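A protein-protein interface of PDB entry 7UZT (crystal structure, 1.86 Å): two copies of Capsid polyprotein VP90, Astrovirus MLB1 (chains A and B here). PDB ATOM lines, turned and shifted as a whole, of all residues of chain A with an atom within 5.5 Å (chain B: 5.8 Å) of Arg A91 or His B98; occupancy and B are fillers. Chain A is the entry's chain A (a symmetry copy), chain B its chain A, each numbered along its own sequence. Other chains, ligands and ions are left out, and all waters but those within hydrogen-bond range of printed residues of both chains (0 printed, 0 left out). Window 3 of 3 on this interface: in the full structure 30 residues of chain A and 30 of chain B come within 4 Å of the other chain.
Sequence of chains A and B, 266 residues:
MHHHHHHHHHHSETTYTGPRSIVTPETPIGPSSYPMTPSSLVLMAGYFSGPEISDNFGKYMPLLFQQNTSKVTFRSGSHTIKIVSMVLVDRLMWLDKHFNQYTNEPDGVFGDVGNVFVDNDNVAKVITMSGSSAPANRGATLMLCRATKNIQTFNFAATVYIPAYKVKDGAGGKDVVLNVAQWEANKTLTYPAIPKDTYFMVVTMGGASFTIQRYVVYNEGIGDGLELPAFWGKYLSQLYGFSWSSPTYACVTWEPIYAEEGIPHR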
ATOM      1  N   ALA A  45      14.604  24.984 -12.935  1.00  0.00           N
ATOM      2  CA  ALA A  45      14.252  24.464 -14.248  1.00  0.00           C
ATOM      3  C   ALA A  45      13.413  23.201 -14.112  1.00  0.00           C
ATOM      4  O   ALA A  45      13.549  22.444 -13.148  1.00  0.00           O
ATOM      5  CB  ALA A  45      15.510  24.167 -15.056  1.00  0.00           C
ATOM      6  N   GLY A  46      12.535  22.982 -15.081  1.00  0.00           N
ATOM      7  CA  GLY A  46      11.799  21.730 -15.145  1.00  0.00           C
ATOM      8  C   GLY A  46      10.554  21.906 -15.988  1.00  0.00           C
ATOM      9  O   GLY A  46      10.426  22.875 -16.736  1.00  0.00           O
ATOM     10  N   TYR A  47       9.639  20.950 -15.848  1.00  0.00           N
ATOM     11  CA  TYR A  47       8.344  21.036 -16.513  1.00  0.00           C
ATOM     12  C   TYR A  47       7.352  21.608 -15.523  1.00  0.00           C
ATOM     13  O   TYR A  47       7.001  20.952 -14.532  1.00  0.00           O
ATOM     14  CB  TYR A  47       7.887  19.680 -17.039  1.00  0.00           C
ATOM     15  CG  TYR A  47       8.697  19.258 -18.254  1.00  0.00           C
ATOM     16  CD1 TYR A  47       9.950  18.689 -18.106  1.00  0.00           C
ATOM     17  CD2 TYR A  47       8.222  19.475 -19.527  1.00  0.00           C
ATOM     18  CE1 TYR A  47      10.707  18.325 -19.203  1.00  0.00           C
ATOM     19  CE2 TYR A  47       8.951  19.115 -20.626  1.00  0.00           C
ATOM     20  CZ  TYR A  47      10.191  18.527 -20.452  1.00  0.00           C
ATOM     21  OH  TYR A  47      10.905  18.168 -21.547  1.00  0.00           O
ATOM     22  N   VAL A  89       6.406  22.003 -10.230  1.00  0.00           N
ATOM     23  CA  VAL A  89       7.528  21.614 -11.087  1.00  0.00           C
ATOM     24  C   VAL A  89       7.754  20.115 -10.987  1.00  0.00           C
ATOM     25  O   VAL A  89       8.087  19.608  -9.911  1.00  0.00           O
ATOM     26  CB  VAL A  89       8.817  22.352 -10.712  1.00  0.00           C
ATOM     27  CG1 VAL A  89       9.832  22.201 -11.808  1.00  0.00           C
ATOM     28  CG2 VAL A  89       8.524  23.817 -10.486  1.00  0.00           C
ATOM     29  N   ASP A  90       7.624  19.414 -12.105  1.00  0.00           N
ATOM     30  CA  ASP A  90       8.203  18.076 -12.208  1.00  0.00           C
ATOM     31  C   ASP A  90       9.625  18.184 -12.735  1.00  0.00           C
ATOM     32  O   ASP A  90       9.974  19.168 -13.381  1.00  0.00           O
ATOM     33  CB  ASP A  90       7.383  17.208 -13.163  1.00  0.00           C
ATOM     34  CG  ASP A  90       5.953  17.030 -12.714  1.00  0.00           C
ATOM     35  OD1 ASP A  90       5.721  16.846 -11.490  1.00  0.00           O
ATOM     36  OD2 ASP A  90       5.058  17.079 -13.590  1.00  0.00           O
ATOM     37  N   ARG A  91      10.449  17.150 -12.456  1.00  0.00           N
ATOM     38  CA  ARG A  91      11.776  17.005 -13.059  1.00  0.00           C
ATOM     39  C   ARG A  91      12.657  18.224 -12.754  1.00  0.00           C
ATOM     40  O   ARG A  91      13.432  18.700 -13.585  1.00  0.00           O
ATOM     41  CB  ARG A  91      11.662  16.750 -14.571  1.00  0.00           C
ATOM     42  CG  ARG A  91      12.832  15.979 -15.185  1.00  0.00           C
ATOM     43  CD  ARG A  91      13.960  16.853 -15.830  1.00  0.00           C
ATOM     44  NE  ARG A  91      13.508  17.824 -16.839  1.00  0.00           N
ATOM     45  CZ  ARG A  91      13.881  19.099 -16.880  1.00  0.00           C
ATOM     46  NH1 ARG A  91      14.673  19.627 -15.957  1.00  0.00           N
ATOM     47  NH2 ARG A  91      13.461  19.865 -17.877  1.00  0.00           N
ATOM     48  N   LEU A  92      12.535  18.713 -11.532  1.00  0.00           N
ATOM     49  CA  LEU A  92      13.211  19.922 -11.098  1.00  0.00           C
ATOM     50  C   LEU A  92      14.733  19.807 -11.176  1.00  0.00           C
ATOM     51  O   LEU A  92      15.328  18.791 -10.810  1.00  0.00           O
ATOM     52  CB  LEU A  92      12.768  20.204  -9.668  1.00  0.00           C
ATOM     53  CG  LEU A  92      13.631  21.051  -8.766  1.00  0.00           C
ATOM     54  CD1 LEU A  92      13.521  22.468  -9.246  1.00  0.00           C
ATOM     55  CD2 LEU A  92      13.108  20.874  -7.333  1.00  0.00           C
ATOM     56  N   MET A  93      15.373  20.874 -11.629  1.00  0.00           N
ATOM     57  CA  MET A  93      16.818  20.982 -11.626  1.00  0.00           C
ATOM     58  C   MET A  93      17.180  22.393 -11.199  1.00  0.00           C
ATOM     59  O   MET A  93      16.575  23.359 -11.660  1.00  0.00           O
ATOM     60  CB  MET A  93      17.410  20.689 -13.010  1.00  0.00           C
ATOM     61  CG  MET A  93      17.118  19.305 -13.539  1.00  0.00           C
ATOM     62  SD  MET A  93      17.585  19.185 -15.277  1.00  0.00           S
ATOM     63  CE  MET A  93      19.027  20.211 -15.313  1.00  0.00           C
ATOM     64  N   PRO A 247       9.903  22.361 -21.503  1.00  0.00           N
ATOM     65  CA  PRO A 247      10.550  22.688 -20.218  1.00  0.00           C
ATOM     66  C   PRO A 247      10.932  24.162 -20.167  1.00  0.00           C
ATOM     67  O   PRO A 247      11.178  24.792 -21.201  1.00  0.00           O
ATOM     68  CB  PRO A 247      11.806  21.802 -20.207  1.00  0.00           C
ATOM     69  CG  PRO A 247      12.096  21.549 -21.648  1.00  0.00           C
ATOM     70  CD  PRO A 247      10.772  21.539 -22.361  1.00  0.00           C
ATOM     71  N   LEU B  43      17.293  20.700 -28.355  1.00  0.00           N
ATOM     72  CA  LEU B  43      17.099  22.106 -28.015  1.00  0.00           C
ATOM     73  C   LEU B  43      18.400  22.858 -28.266  1.00  0.00           C
ATOM     74  O   LEU B  43      19.489  22.386 -27.939  1.00  0.00           O
ATOM     75  CB  LEU B  43      16.663  22.256 -26.548  1.00  0.00           C
ATOM     76  CG  LEU B  43      15.420  21.437 -26.136  1.00  0.00           C
ATOM     77  CD1 LEU B  43      15.049  21.603 -24.663  1.00  0.00           C
ATOM     78  CD2 LEU B  43      14.203  21.795 -27.053  1.00  0.00           C
ATOM     79  N   ASP B  96      18.827  17.943 -24.544  1.00  0.00           N
ATOM     80  CA  ASP B  96      17.641  17.149 -24.803  1.00  0.00           C
ATOM     81  C   ASP B  96      16.487  17.679 -23.954  1.00  0.00           C
ATOM     82  O   ASP B  96      16.636  18.666 -23.217  1.00  0.00           O
ATOM     83  CB  ASP B  96      17.937  15.671 -24.560  1.00  0.00           C
ATOM     84  CG  ASP B  96      18.193  15.349 -23.097  1.00  0.00           C
ATOM     85  OD1 ASP B  96      18.135  16.250 -22.220  1.00  0.00           O
ATOM     86  OD2 ASP B  96      18.521  14.182 -22.841  1.00  0.00           O
ATOM     87  N   LYS B  97      15.321  17.028 -24.032  1.00  0.00           N
ATOM     88  CA  LYS B  97      14.094  17.496 -23.329  1.00  0.00           C
ATOM     89  C   LYS B  97      14.300  17.576 -21.807  1.00  0.00           C
ATOM     90  O   LYS B  97      13.481  18.185 -21.129  1.00  0.00           O
ATOM     91  CB  LYS B  97      12.940  16.552 -23.664  1.00  0.00           C
ATOM     92  CG  LYS B  97      13.102  15.120 -23.185  1.00  0.00           C
ATOM     93  CD  LYS B  97      12.285  14.128 -23.982  1.00  0.00           C
ATOM     94  CE  LYS B  97      13.117  13.296 -24.934  1.00  0.00           C
ATOM     95  NZ  LYS B  97      14.476  13.026 -24.404  1.00  0.00           N
ATOM     96  N   HIS B  98      15.352  16.944 -21.310  1.00  0.00           N
ATOM     97  CA  HIS B  98      15.591  16.939 -19.873  1.00  0.00           C
ATOM     98  C   HIS B  98      16.775  17.837 -19.505  1.00  0.00           C
ATOM     99  O   HIS B  98      17.283  17.775 -18.375  1.00  0.00           O
ATOM    100  CB  HIS B  98      15.813  15.496 -19.427  1.00  0.00           C
ATOM    101  CG  HIS B  98      14.573  14.661 -19.517  1.00  0.00           C
ATOM    102  ND1 HIS B  98      14.548  13.436 -20.149  1.00  0.00           N
ATOM    103  CD2 HIS B  98      13.310  14.889 -19.085  1.00  0.00           C
ATOM    104  CE1 HIS B  98      13.327  12.938 -20.087  1.00  0.00           C
ATOM    105  NE2 HIS B  98      12.555  13.800 -19.448  1.00  0.00           N
ATOM    106  N   PHE B  99      17.222  18.669 -20.446  1.00  0.00           N
ATOM    107  CA  PHE B  99      18.341  19.603 -20.294  1.00  0.00           C
ATOM    108  C   PHE B  99      19.674  18.901 -20.077  1.00  0.00           C
ATOM    109  O   PHE B  99      20.611  19.507 -19.551  1.00  0.00           O
ATOM    110  CB  PHE B  99      18.090  20.629 -19.179  1.00  0.00           C
ATOM    111  CG  PHE B  99      17.087  21.695 -19.541  1.00  0.00           C
ATOM    112  CD1 PHE B  99      16.611  21.803 -20.836  1.00  0.00           C
ATOM    113  CD2 PHE B  99      16.617  22.577 -18.582  1.00  0.00           C
ATOM    114  CE1 PHE B  99      15.686  22.775 -21.163  1.00  0.00           C
ATOM    115  CE2 PHE B  99      15.696  23.545 -18.892  1.00  0.00           C
ATOM    116  CZ  PHE B  99      15.233  23.653 -20.198  1.00  0.00           C
ATOM    117  N   ASN B 100      19.798  17.646 -20.520  1.00  0.00           N
ATOM    118  CA  ASN B 100      21.077  16.950 -20.559  1.00  0.00           C
ATOM    119  C   ASN B 100      21.794  17.279 -21.861  1.00  0.00           C
ATOM    120  O   ASN B 100      21.175  17.364 -22.920  1.00  0.00           O
ATOM    121  CB  ASN B 100      20.863  15.443 -20.412  1.00  0.00           C
ATOM    122  CG  ASN B 100      19.929  15.120 -19.268  1.00  0.00           C
ATOM    123  OD1 ASN B 100      19.191  14.136 -19.332  1.00  0.00           O
ATOM    124  ND2 ASN B 100      19.980  15.913 -18.206  1.00  0.00           N
ATOM    125  N   TYR B 258       7.334  16.684 -26.011  1.00  0.00           N
ATOM    126  CA  TYR B 258       8.013  16.812 -24.728  1.00  0.00           C
ATOM    127  C   TYR B 258       7.567  15.775 -23.717  1.00  0.00           C
ATOM    128  O   TYR B 258       8.331  15.445 -22.802  1.00  0.00           O
ATOM    129  CB  TYR B 258       7.793  18.210 -24.176  1.00  0.00           C
ATOM    130  CG  TYR B 258       8.498  19.221 -25.009  1.00  0.00           C
ATOM    131  CD1 TYR B 258       9.882  19.368 -24.931  1.00  0.00           C
ATOM    132  CD2 TYR B 258       7.787  20.023 -25.902  1.00  0.00           C
ATOM    133  CE1 TYR B 258      10.521  20.286 -25.692  1.00  0.00           C
ATOM    134  CE2 TYR B 258       8.431  20.942 -26.684  1.00  0.00           C
ATOM    135  CZ  TYR B 258       9.797  21.061 -26.587  1.00  0.00           C
ATOM    136  OH  TYR B 258      10.440  21.996 -27.367  1.00  0.00           O
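No position is printed for both chains. Of the 10 pairs that touch across the chains among the printed residues, none has its exchanged pair printed and touching as well.
Among the printed residues, no Asp or Glu carboxylate lies within 4 Å of a Lys or Arg side-chain nitrogen of the other chain.
Arg A91 touches two residues of chain B. Leu A92 touches none of the printed residues of chain B. Printed residues of chain B within 4 Å of Met A93: His B98 (3.4 Å) and Phe B99 (3.9998 Å). Printed residues of chain B within 4 Å of Pro A247: Lys B97, Phe B99 and Tyr B258. Printed residues of chain A within 4 Å of Lys B97: Tyr A47, Arg A91 and Pro A247. His B98 touches two residues of chain A. Of the printed residues of chain A, Phe B99 touches Ala A45 (3.9 Å), Met A93 (3.9998 Å) and Pro A247 (3.8 Å). The nearest residue of chain B that does not touch Arg A91 is Phe B99 (4.2 Å). The nearest residue of chain A that does not touch His B98 is Tyr A47 (4.3 Å).
The guanidinium group (NH1) of Arg A91 lies within hydrogen-bond range of the side-chain sulfur (SD) of Met A93 (3.0 Å). The side-chain carboxylate of Asp B96 lies close to the backbone NH of His B98 (3.0 Å). O of His B98 is in hydrogen-bond range of ND2 of Asn B100, 3.3 Å away. The backbone carbonyl oxygen of Ala A45 is in hydrogen-bond range of the backbone NH of Met A93 (2.8 Å). The backbone carbonyl oxygen (O) of Tyr A47 lies within hydrogen-bond range of the backbone NH (N) of Asp A90 (2.9 Å). The side-chain carboxylate (OD1) of Asp B96 sits at hydrogen-bond distance from the backbone NH (N) of Phe B99.
Among the printed residues, pairs that only touch across the chains: Pro A247 with Tyr B258, Arg A91 with Lys B97, Pro A247 with Lys B97, Arg A91 with His B98, Tyr A47 with Tyr B258, Pro A247 with Phe B99, Ala A45 with Phe B99 and Met A93 with Phe B99.
O of Lys B97 lies within hydrogen-bond range of OH of Tyr A47 (2.6 Å). The side-chain sulfur of Met A93 sits close to the backbone carbonyl oxygen of His B98 (3.4 Å).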
